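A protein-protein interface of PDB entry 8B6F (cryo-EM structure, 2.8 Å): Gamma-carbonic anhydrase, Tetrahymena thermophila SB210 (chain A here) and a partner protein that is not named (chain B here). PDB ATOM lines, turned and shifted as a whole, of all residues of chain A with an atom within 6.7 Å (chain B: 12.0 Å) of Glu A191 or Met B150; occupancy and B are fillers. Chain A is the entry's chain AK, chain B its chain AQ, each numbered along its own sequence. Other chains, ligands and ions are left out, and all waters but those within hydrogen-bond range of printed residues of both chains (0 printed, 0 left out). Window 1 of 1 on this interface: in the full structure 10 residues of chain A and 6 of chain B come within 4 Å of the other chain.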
ATOM      1  N   MET A 157      20.411 -37.389 -30.218  1.00  0.00           N
ATOM      2  CA  MET A 157      20.492 -36.270 -31.142  1.00  0.00           C
ATOM      3  C   MET A 157      21.283 -36.685 -32.372  1.00  0.00           C
ATOM      4  O   MET A 157      22.159 -37.550 -32.301  1.00  0.00           O
ATOM      5  CB  MET A 157      21.159 -35.050 -30.498  1.00  0.00           C
ATOM      6  CG  MET A 157      20.300 -34.351 -29.463  1.00  0.00           C
ATOM      7  SD  MET A 157      21.044 -32.831 -28.844  1.00  0.00           S
ATOM      8  CE  MET A 157      21.045 -31.818 -30.318  1.00  0.00           C
ATOM      9  N   ALA A 159      23.215 -34.974 -35.971  1.00  0.00           N
ATOM     10  CA  ALA A 159      23.666 -33.773 -36.653  1.00  0.00           C
ATOM     11  C   ALA A 159      22.849 -33.542 -37.923  1.00  0.00           C
ATOM     12  O   ALA A 159      22.144 -34.426 -38.412  1.00  0.00           O
ATOM     13  CB  ALA A 159      25.152 -33.870 -36.987  1.00  0.00           C
ATOM     14  N   LEU A 175      24.926 -38.428 -28.832  1.00  0.00           N
ATOM     15  CA  LEU A 175      25.065 -37.533 -29.972  1.00  0.00           C
ATOM     16  C   LEU A 175      25.802 -38.251 -31.093  1.00  0.00           C
ATOM     17  O   LEU A 175      26.844 -38.870 -30.857  1.00  0.00           O
ATOM     18  CB  LEU A 175      25.816 -36.261 -29.574  1.00  0.00           C
ATOM     19  CG  LEU A 175      26.010 -35.202 -30.661  1.00  0.00           C
ATOM     20  CD1 LEU A 175      24.676 -34.693 -31.177  1.00  0.00           C
ATOM     21  CD2 LEU A 175      26.852 -34.057 -30.135  1.00  0.00           C
ATOM     22  N   VAL A 184      29.740 -39.230 -30.897  1.00  0.00           N
ATOM     23  CA  VAL A 184      30.480 -38.029 -30.527  1.00  0.00           C
ATOM     24  C   VAL A 184      30.670 -37.991 -29.016  1.00  0.00           C
ATOM     25  O   VAL A 184      31.802 -37.957 -28.523  1.00  0.00           O
ATOM     26  CB  VAL A 184      29.758 -36.761 -31.021  1.00  0.00           C
ATOM     27  CG1 VAL A 184      30.526 -35.510 -30.623  1.00  0.00           C
ATOM     28  CG2 VAL A 184      29.565 -36.808 -32.527  1.00  0.00           C
ATOM     29  N   ARG A 185      29.568 -37.991 -28.271  1.00  0.00           N
ATOM     30  CA  ARG A 185      29.630 -37.941 -26.816  1.00  0.00           C
ATOM     31  C   ARG A 185      28.232 -38.182 -26.267  1.00  0.00           C
ATOM     32  O   ARG A 185      27.254 -38.260 -27.014  1.00  0.00           O
ATOM     33  CB  ARG A 185      30.176 -36.600 -26.318  1.00  0.00           C
ATOM     34  CG  ARG A 185      29.307 -35.403 -26.680  1.00  0.00           C
ATOM     35  CD  ARG A 185      29.874 -34.116 -26.108  1.00  0.00           C
ATOM     36  NE  ARG A 185      29.056 -32.958 -26.449  1.00  0.00           N
ATOM     37  CZ  ARG A 185      27.998 -32.553 -25.759  1.00  0.00           C
ATOM     38  NH1 ARG A 185      27.586 -33.200 -24.682  1.00  0.00           N
ATOM     39  NH2 ARG A 185      27.338 -31.472 -26.160  1.00  0.00           N
ATOM     40  N   ASN A 186      28.153 -38.306 -24.946  1.00  0.00           N
ATOM     41  CA  ASN A 186      26.873 -38.412 -24.269  1.00  0.00           C
ATOM     42  C   ASN A 186      26.255 -37.030 -24.072  1.00  0.00           C
ATOM     43  O   ASN A 186      26.945 -36.007 -24.059  1.00  0.00           O
ATOM     44  CB  ASN A 186      27.029 -39.105 -22.916  1.00  0.00           C
ATOM     45  CG  ASN A 186      27.496 -40.535 -23.048  1.00  0.00           C
ATOM     46  OD1 ASN A 186      27.212 -41.204 -24.039  1.00  0.00           O
ATOM     47  ND2 ASN A 186      28.220 -41.015 -22.045  1.00  0.00           N
ATOM     48  N   LEU A 187      24.937 -37.014 -23.913  1.00  0.00           N
ATOM     49  CA  LEU A 187      24.184 -35.788 -23.700  1.00  0.00           C
ATOM     50  C   LEU A 187      23.789 -35.682 -22.234  1.00  0.00           C
ATOM     51  O   LEU A 187      23.433 -36.681 -21.603  1.00  0.00           O
ATOM     52  CB  LEU A 187      22.939 -35.750 -24.589  1.00  0.00           C
ATOM     53  CG  LEU A 187      23.205 -35.689 -26.094  1.00  0.00           C
ATOM     54  CD1 LEU A 187      21.914 -35.855 -26.863  1.00  0.00           C
ATOM     55  CD2 LEU A 187      23.883 -34.385 -26.480  1.00  0.00           C
ATOM     56  N   THR A 188      23.853 -34.468 -21.698  1.00  0.00           N
ATOM     57  CA  THR A 188      23.583 -34.226 -20.290  1.00  0.00           C
ATOM     58  C   THR A 188      22.117 -33.863 -20.073  1.00  0.00           C
ATOM     59  O   THR A 188      21.382 -33.536 -21.005  1.00  0.00           O
ATOM     60  CB  THR A 188      24.483 -33.111 -19.756  1.00  0.00           C
ATOM     61  OG1 THR A 188      24.270 -31.914 -20.514  1.00  0.00           O
ATOM     62  CG2 THR A 188      25.943 -33.513 -19.850  1.00  0.00           C
ATOM     63  N   LYS A 189      21.697 -33.921 -18.807  1.00  0.00           N
ATOM     64  CA  LYS A 189      20.319 -33.578 -18.468  1.00  0.00           C
ATOM     65  C   LYS A 189      19.970 -32.166 -18.913  1.00  0.00           C
ATOM     66  O   LYS A 189      18.822 -31.899 -19.285  1.00  0.00           O
ATOM     67  CB  LYS A 189      20.096 -33.732 -16.966  1.00  0.00           C
ATOM     68  CG  LYS A 189      20.327 -35.141 -16.451  1.00  0.00           C
ATOM     69  CD  LYS A 189      19.892 -35.270 -15.001  1.00  0.00           C
ATOM     70  CE  LYS A 189      20.146 -36.669 -14.466  1.00  0.00           C
ATOM     71  NZ  LYS A 189      21.599 -36.996 -14.426  1.00  0.00           N
ATOM     72  N   SER A 190      20.937 -31.250 -18.878  1.00  0.00           N
ATOM     73  CA  SER A 190      20.684 -29.897 -19.356  1.00  0.00           C
ATOM     74  C   SER A 190      20.354 -29.895 -20.844  1.00  0.00           C
ATOM     75  O   SER A 190      19.429 -29.201 -21.280  1.00  0.00           O
ATOM     76  CB  SER A 190      21.889 -29.003 -19.069  1.00  0.00           C
ATOM     77  OG  SER A 190      23.063 -29.528 -19.659  1.00  0.00           O
ATOM     78  N   GLU A 191      21.103 -30.660 -21.641  1.00  0.00           N
ATOM     79  CA  GLU A 191      20.810 -30.734 -23.069  1.00  0.00           C
ATOM     80  C   GLU A 191      19.440 -31.350 -23.315  1.00  0.00           C
ATOM     81  O   GLU A 191      18.680 -30.873 -24.165  1.00  0.00           O
ATOM     82  CB  GLU A 191      21.892 -31.541 -23.786  1.00  0.00           C
ATOM     83  CG  GLU A 191      23.299 -31.003 -23.599  1.00  0.00           C
ATOM     84  CD  GLU A 191      23.492 -29.635 -24.226  1.00  0.00           C
ATOM     85  OE1 GLU A 191      22.567 -29.157 -24.917  1.00  0.00           O
ATOM     86  OE2 GLU A 191      24.572 -29.038 -24.032  1.00  0.00           O
ATOM     87  N   LEU A 192      19.108 -32.415 -22.586  1.00  0.00           N
ATOM     88  CA  LEU A 192      17.800 -33.042 -22.746  1.00  0.00           C
ATOM     89  C   LEU A 192      16.684 -32.072 -22.380  1.00  0.00           C
ATOM     90  O   LEU A 192      15.662 -31.997 -23.072  1.00  0.00           O
ATOM     91  CB  LEU A 192      17.715 -34.309 -21.899  1.00  0.00           C
ATOM     92  CG  LEU A 192      18.810 -35.350 -22.144  1.00  0.00           C
ATOM     93  CD1 LEU A 192      18.633 -36.532 -21.210  1.00  0.00           C
ATOM     94  CD2 LEU A 192      18.816 -35.811 -23.591  1.00  0.00           C
ATOM     95  N   ALA A 193      16.860 -31.327 -21.289  1.00  0.00           N
ATOM     96  CA  ALA A 193      15.860 -30.344 -20.893  1.00  0.00           C
ATOM     97  C   ALA A 193      15.713 -29.254 -21.945  1.00  0.00           C
ATOM     98  O   ALA A 193      14.600 -28.792 -22.221  1.00  0.00           O
ATOM     99  CB  ALA A 193      16.231 -29.735 -19.543  1.00  0.00           C
ATOM    100  N   THR A 194      16.826 -28.822 -22.537  1.00  0.00           N
ATOM    101  CA  THR A 194      16.753 -27.812 -23.587  1.00  0.00           C
ATOM    102  C   THR A 194      15.966 -28.322 -24.786  1.00  0.00           C
ATOM    103  O   THR A 194      15.143 -27.593 -25.350  1.00  0.00           O
ATOM    104  CB  THR A 194      18.161 -27.400 -24.016  1.00  0.00           C
ATOM    105  OG1 THR A 194      18.917 -26.996 -22.869  1.00  0.00           O
ATOM    106  CG2 THR A 194      18.102 -26.249 -25.005  1.00  0.00           C
ATOM    107  N   ASN A 195      16.203 -29.570 -25.193  1.00  0.00           N
ATOM    108  CA  ASN A 195      15.464 -30.130 -26.319  1.00  0.00           C
ATOM    109  C   ASN A 195      13.975 -30.202 -26.011  1.00  0.00           C
ATOM    110  O   ASN A 195      13.138 -29.829 -26.840  1.00  0.00           O
ATOM    111  CB  ASN A 195      16.007 -31.516 -26.664  1.00  0.00           C
ATOM    112  CG  ASN A 195      17.479 -31.492 -27.011  1.00  0.00           C
ATOM    113  OD1 ASN A 195      18.012 -30.467 -27.432  1.00  0.00           O
ATOM    114  ND2 ASN A 195      18.146 -32.625 -26.836  1.00  0.00           N
ATOM    115  N   ILE A 196      13.624 -30.672 -24.814  1.00  0.00           N
ATOM    116  CA  ILE A 196      12.216 -30.745 -24.428  1.00  0.00           C
ATOM    117  C   ILE A 196      11.602 -29.353 -24.423  1.00  0.00           C
ATOM    118  O   ILE A 196      10.455 -29.161 -24.841  1.00  0.00           O
ATOM    119  CB  ILE A 196      12.072 -31.432 -23.058  1.00  0.00           C
ATOM    120  CG1 ILE A 196      12.568 -32.875 -23.133  1.00  0.00           C
ATOM    121  CG2 ILE A 196      10.620 -31.403 -22.595  1.00  0.00           C
ATOM    122  CD1 ILE A 196      12.690 -33.552 -21.781  1.00  0.00           C
ATOM    123  N   GLU B 143      27.407 -16.629 -24.743  1.00  0.00           N
ATOM    124  CA  GLU B 143      27.770 -17.266 -23.482  1.00  0.00           C
ATOM    125  C   GLU B 143      28.798 -18.373 -23.672  1.00  0.00           C
ATOM    126  O   GLU B 143      29.738 -18.500 -22.879  1.00  0.00           O
ATOM    127  CB  GLU B 143      26.517 -17.819 -22.803  1.00  0.00           C
ATOM    128  CG  GLU B 143      25.502 -16.754 -22.426  1.00  0.00           C
ATOM    129  CD  GLU B 143      24.321 -17.328 -21.672  1.00  0.00           C
ATOM    130  OE1 GLU B 143      24.193 -18.568 -21.627  1.00  0.00           O
ATOM    131  OE2 GLU B 143      23.522 -16.541 -21.120  1.00  0.00           O
ATOM    132  N   ASN B 144      28.648 -19.173 -24.722  1.00  0.00           N
ATOM    133  CA  ASN B 144      29.483 -20.345 -24.934  1.00  0.00           C
ATOM    134  C   ASN B 144      29.986 -20.369 -26.369  1.00  0.00           C
ATOM    135  O   ASN B 144      29.540 -19.600 -27.224  1.00  0.00           O
ATOM    136  CB  ASN B 144      28.713 -21.635 -24.622  1.00  0.00           C
ATOM    137  CG  ASN B 144      27.408 -21.732 -25.389  1.00  0.00           C
ATOM    138  OD1 ASN B 144      27.339 -22.363 -26.442  1.00  0.00           O
ATOM    139  ND2 ASN B 144      26.364 -21.102 -24.863  1.00  0.00           N
ATOM    140  N   ARG B 145      30.940 -21.267 -26.620  1.00  0.00           N
ATOM    141  CA  ARG B 145      31.436 -21.508 -27.964  1.00  0.00           C
ATOM    142  C   ARG B 145      30.733 -22.735 -28.520  1.00  0.00           C
ATOM    143  O   ARG B 145      30.987 -23.848 -28.037  1.00  0.00           O
ATOM    144  CB  ARG B 145      32.946 -21.725 -27.953  1.00  0.00           C
ATOM    145  CG  ARG B 145      33.755 -20.500 -27.572  1.00  0.00           C
ATOM    146  CD  ARG B 145      33.583 -19.381 -28.580  1.00  0.00           C
ATOM    147  NE  ARG B 145      34.675 -18.419 -28.517  1.00  0.00           N
ATOM    148  CZ  ARG B 145      34.747 -17.316 -29.251  1.00  0.00           C
ATOM    149  NH1 ARG B 145      33.789 -16.990 -30.102  1.00  0.00           N
ATOM    150  NH2 ARG B 145      35.807 -16.523 -29.129  1.00  0.00           N
ATOM    151  N   PRO B 146      29.858 -22.602 -29.516  1.00  0.00           N
ATOM    152  CA  PRO B 146      29.150 -23.781 -30.021  1.00  0.00           C
ATOM    153  C   PRO B 146      30.116 -24.788 -30.623  1.00  0.00           C
ATOM    154  O   PRO B 146      31.105 -24.426 -31.261  1.00  0.00           O
ATOM    155  CB  PRO B 146      28.205 -23.202 -31.078  1.00  0.00           C
ATOM    156  CG  PRO B 146      28.885 -21.964 -31.536  1.00  0.00           C
ATOM    157  CD  PRO B 146      29.571 -21.404 -30.326  1.00  0.00           C
ATOM    158  N   GLU B 147      29.816 -26.064 -30.418  1.00  0.00           N
ATOM    159  CA  GLU B 147      30.592 -27.146 -30.998  1.00  0.00           C
ATOM    160  C   GLU B 147      29.866 -27.705 -32.212  1.00  0.00           C
ATOM    161  O   GLU B 147      28.637 -27.663 -32.299  1.00  0.00           O
ATOM    162  CB  GLU B 147      30.839 -28.257 -29.976  1.00  0.00           C
ATOM    163  CG  GLU B 147      29.583 -28.983 -29.525  1.00  0.00           C
ATOM    164  CD  GLU B 147      29.873 -30.041 -28.478  1.00  0.00           C
ATOM    165  OE1 GLU B 147      30.943 -29.964 -27.838  1.00  0.00           O
ATOM    166  OE2 GLU B 147      29.038 -30.950 -28.297  1.00  0.00           O
ATOM    167  N   GLU B 148      30.643 -28.223 -33.158  1.00  0.00           N
ATOM    168  CA  GLU B 148      30.058 -28.806 -34.355  1.00  0.00           C
ATOM    169  C   GLU B 148      29.162 -29.977 -33.974  1.00  0.00           C
ATOM    170  O   GLU B 148      29.443 -30.709 -33.021  1.00  0.00           O
ATOM    171  CB  GLU B 148      31.159 -29.263 -35.310  1.00  0.00           C
ATOM    172  CG  GLU B 148      32.062 -28.134 -35.780  1.00  0.00           C
ATOM    173  CD  GLU B 148      33.251 -28.630 -36.575  1.00  0.00           C
ATOM    174  OE1 GLU B 148      33.571 -29.833 -36.483  1.00  0.00           O
ATOM    175  OE2 GLU B 148      33.866 -27.815 -37.294  1.00  0.00           O
ATOM    176  N   ALA B 149      28.067 -30.135 -34.713  1.00  0.00           N
ATOM    177  CA  ALA B 149      27.060 -31.169 -34.493  1.00  0.00           C
ATOM    178  C   ALA B 149      26.165 -30.870 -33.299  1.00  0.00           C
ATOM    179  O   ALA B 149      25.508 -31.778 -32.783  1.00  0.00           O
ATOM    180  CB  ALA B 149      27.690 -32.556 -34.318  1.00  0.00           C
ATOM    181  N   MET B 150      26.124 -29.624 -32.837  1.00  0.00           N
ATOM    182  CA  MET B 150      25.239 -29.214 -31.760  1.00  0.00           C
ATOM    183  C   MET B 150      24.643 -27.852 -32.088  1.00  0.00           C
ATOM    184  O   MET B 150      25.299 -27.026 -32.733  1.00  0.00           O
ATOM    185  CB  MET B 150      25.976 -29.127 -30.415  1.00  0.00           C
ATOM    186  CG  MET B 150      26.283 -30.472 -29.785  1.00  0.00           C
ATOM    187  SD  MET B 150      24.806 -31.395 -29.316  1.00  0.00           S
ATOM    188  CE  MET B 150      24.085 -30.312 -28.089  1.00  0.00           C
ATOM    189  N   PRO B 151      23.410 -27.589 -31.660  1.00  0.00           N
ATOM    190  CA  PRO B 151      22.852 -26.243 -31.818  1.00  0.00           C
ATOM    191  C   PRO B 151      23.527 -25.250 -30.884  1.00  0.00           C
ATOM    192  O   PRO B 151      24.221 -25.615 -29.934  1.00  0.00           O
ATOM    193  CB  PRO B 151      21.370 -26.417 -31.462  1.00  0.00           C
ATOM    194  CG  PRO B 151      21.113 -27.878 -31.539  1.00  0.00           C
ATOM    195  CD  PRO B 151      22.397 -28.541 -31.173  1.00  0.00           C
ATOM    196  N   PHE B 152      23.313 -23.972 -31.177  1.00  0.00           N
ATOM    197  CA  PHE B 152      23.841 -22.885 -30.360  1.00  0.00           C
ATOM    198  C   PHE B 152      22.783 -22.492 -29.337  1.00  0.00           C
ATOM    199  O   PHE B 152      21.787 -21.846 -29.681  1.00  0.00           O
ATOM    200  CB  PHE B 152      24.235 -21.698 -31.235  1.00  0.00           C
ATOM    201  CG  PHE B 152      24.775 -20.530 -30.463  1.00  0.00           C
ATOM    202  CD1 PHE B 152      23.928 -19.543 -29.993  1.00  0.00           C
ATOM    203  CD2 PHE B 152      26.129 -20.415 -30.215  1.00  0.00           C
ATOM    204  CE1 PHE B 152      24.422 -18.468 -29.285  1.00  0.00           C
ATOM    205  CE2 PHE B 152      26.630 -19.343 -29.508  1.00  0.00           C
ATOM    206  CZ  PHE B 152      25.776 -18.368 -29.042  1.00  0.00           C
ATOM    207  N   TYR B 153      22.993 -22.883 -28.083  1.00  0.00           N
ATOM    208  CA  TYR B 153      22.083 -22.563 -26.994  1.00  0.00           C
ATOM    209  C   TYR B 153      22.816 -21.792 -25.906  1.00  0.00           C
ATOM    210  O   TYR B 153      24.008 -22.006 -25.663  1.00  0.00           O
ATOM    211  CB  TYR B 153      21.464 -23.829 -26.392  1.00  0.00           C
ATOM    212  CG  TYR B 153      20.338 -24.412 -27.209  1.00  0.00           C
ATOM    213  CD1 TYR B 153      19.164 -23.701 -27.414  1.00  0.00           C
ATOM    214  CD2 TYR B 153      20.437 -25.684 -27.755  1.00  0.00           C
ATOM    215  CE1 TYR B 153      18.129 -24.231 -28.152  1.00  0.00           C
ATOM    216  CE2 TYR B 153      19.406 -26.224 -28.494  1.00  0.00           C
ATOM    217  CZ  TYR B 153      18.254 -25.492 -28.688  1.00  0.00           C
ATOM    218  OH  TYR B 153      17.223 -26.027 -29.424  1.00  0.00           O
ATOM    219  N   GLU B 154      22.088 -20.892 -25.255  1.00  0.00           N
ATOM    220  CA  GLU B 154      22.643 -20.144 -24.136  1.00  0.00           C
ATOM    221  C   GLU B 154      22.904 -21.074 -22.958  1.00  0.00           C
ATOM    222  O   GLU B 154      22.145 -22.014 -22.707  1.00  0.00           O
ATOM    223  CB  GLU B 154      21.685 -19.032 -23.710  1.00  0.00           C
ATOM    224  CG  GLU B 154      21.235 -18.122 -24.839  1.00  0.00           C
ATOM    225  CD  GLU B 154      20.188 -17.124 -24.386  1.00  0.00           C
ATOM    226  OE1 GLU B 154      19.997 -16.984 -23.161  1.00  0.00           O
ATOM    227  OE2 GLU B 154      19.554 -16.485 -25.252  1.00  0.00           O
ATOM    228  N   ASP B 155      23.985 -20.810 -22.232  1.00  0.00           N
ATOM    229  CA  ASP B 155      24.258 -21.557 -21.016  1.00  0.00           C
ATOM    230  C   ASP B 155      23.206 -21.247 -19.958  1.00  0.00           C
ATOM    231  O   ASP B 155      22.681 -20.135 -19.877  1.00  0.00           O
ATOM    232  CB  ASP B 155      25.648 -21.221 -20.473  1.00  0.00           C
ATOM    233  CG  ASP B 155      26.762 -21.759 -21.347  1.00  0.00           C
ATOM    234  OD1 ASP B 155      26.562 -22.808 -21.994  1.00  0.00           O
ATOM    235  OD2 ASP B 155      27.842 -21.132 -21.385  1.00  0.00           O
ATOM    236  N   TYR B 156      22.892 -22.248 -19.149  1.00  0.00           N
ATOM    237  CA  TYR B 156      21.948 -22.045 -18.061  1.00  0.00           C
ATOM    238  C   TYR B 156      22.540 -21.063 -17.057  1.00  0.00           C
ATOM    239  O   TYR B 156      23.669 -21.266 -16.593  1.00  0.00           O
ATOM    240  CB  TYR B 156      21.620 -23.368 -17.380  1.00  0.00           C
ATOM    241  CG  TYR B 156      20.495 -24.128 -18.038  1.00  0.00           C
ATOM    242  CD1 TYR B 156      19.174 -23.880 -17.695  1.00  0.00           C
ATOM    243  CD2 TYR B 156      20.753 -25.093 -18.999  1.00  0.00           C
ATOM    244  CE1 TYR B 156      18.139 -24.570 -18.291  1.00  0.00           C
ATOM    245  CE2 TYR B 156      19.726 -25.791 -19.602  1.00  0.00           C
ATOM    246  CZ  TYR B 156      18.421 -25.524 -19.243  1.00  0.00           C
ATOM    247  OH  TYR B 156      17.392 -26.213 -19.838  1.00  0.00           O
ATOM    248  N   PRO B 157      21.828 -19.998 -16.698  1.00  0.00           N
ATOM    249  CA  PRO B 157      22.391 -19.030 -15.752  1.00  0.00           C
ATOM    250  C   PRO B 157      22.528 -19.620 -14.361  1.00  0.00           C
ATOM    251  O   PRO B 157      21.821 -20.557 -13.981  1.00  0.00           O
ATOM    252  CB  PRO B 157      21.376 -17.883 -15.773  1.00  0.00           C
ATOM    253  CG  PRO B 157      20.098 -18.530 -16.145  1.00  0.00           C
ATOM    254  CD  PRO B 157      20.452 -19.643 -17.088  1.00  0.00           C
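Met A157 touches just these residues of chain B: Met B150 (3.9 Å) and Pro B151 (3.6 Å).
Of the printed residues of chain B, Ala A159 touches Ala B149.
Of the printed residues of chain B, Leu A175 touches Ala B149 and Met B150.
Leu A187 touches none of the printed residues of chain B.
No residue of chain B comes within 4 Å of Thr A188.
Ser A190 touches just one residue of chain B: Tyr B156 (3.8 Å).
Printed residues of chain B within 4 Å of Glu A191: Met B150 (3.7 Å).
No residue of chain B comes within 4 Å of Leu A192.
Thr A194 touches just these residues of chain B: Tyr B153 (3.6 Å) and Tyr B156 (3.5 Å).
Glu B143 touches none of the printed residues of chain A.
Of chain A, only Met A157, Leu A175, Arg A185 and Glu A191 come within 4 Å of Met B150.
Of the printed residues of chain A, Pro B151 touches Met A157 (3.6 Å).
Of the printed residues of chain A, Tyr B153 touches Thr A194 (3.6 Å).
Printed residues of chain A within 4 Å of Tyr B156: Ser A190 (3.8 Å), Ala A193 (3.7 Å) and Thr A194 (3.5 Å).
The nearest residue of chain B that does not touch Glu A191 is Tyr B153 (5.0 Å).
The nearest printed residue of chain B that does not touch Arg A185 is Ala B149 (6.9 Å).
Among the printed residues, merely in contact across the chains: Leu A175 with Ala B149, Leu A175 with Met B150, Thr A194 with Tyr B153, Met A157 with Pro B151, Glu A191 with Met B150, Ala A193 with Tyr B156, Ser A190 with Tyr B156, Arg A185 with Met B150, Ala A159 with Ala B149 and Met A157 with Met B150.
Of the 16 printed residues of chain A, 8 touch a printed residue of chain B.
Printed residues of chain A that touch a printed residue of chain B: Met A157, Ala A159, Leu A175, Arg A185, Ser A190, Glu A191, Ala A193 and Thr A194.
Hydrophobic or aromatic side chains of chain A that line the printed part of chain B: Met A157, Ala A159, Leu A175 and Ala A193.
Printed residues of chain B that touch a printed residue of chain A: Glu B147, Ala B149, Met B150, Pro B151, Tyr B153 and Tyr B156.
Among the printed residues, Asp or Glu carboxylates within 4 Å of a Lys or Arg side-chain nitrogen of the other chain: Arg A185 with Glu B147 (2.7 Å).
The backbone NH of Val A184 sits at hydrogen-bond distance from the backbone carbonyl oxygen of Leu A175, 2.9 Å away.
The backbone carbonyl oxygen (O) of Arg A185 sits at hydrogen-bond distance from the backbone NH (N) of Leu A175, at 3.0 Å.
OG1 of Thr A194 is in hydrogen-bond range of O of Ser A190 (2.8 Å).
The backbone carbonyl oxygen (O) of Tyr B153 sits at hydrogen-bond distance from the side-chain amide nitrogen (ND2) of Asn B144, 2.6 Å away.
The side-chain hydroxyl (OG) of Ser A190 is in hydrogen-bond range of the side-chain hydroxyl (OG1) of Thr A188.
The side-chain amide nitrogen (ND2) of Asn A195 lies within hydrogen-bond range of the side-chain sulfur (SD) of Met A157, 3.5 Å away.
The side-chain hydroxyl of Tyr B156 sits at hydrogen-bond distance from the side-chain hydroxyl of Thr A194 (3.5 Å).
The guanidinium group (NE) of Arg A185 is in salt-bridge range of the side-chain carboxylate (OE2) of Glu B147, 2.7 Å away.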
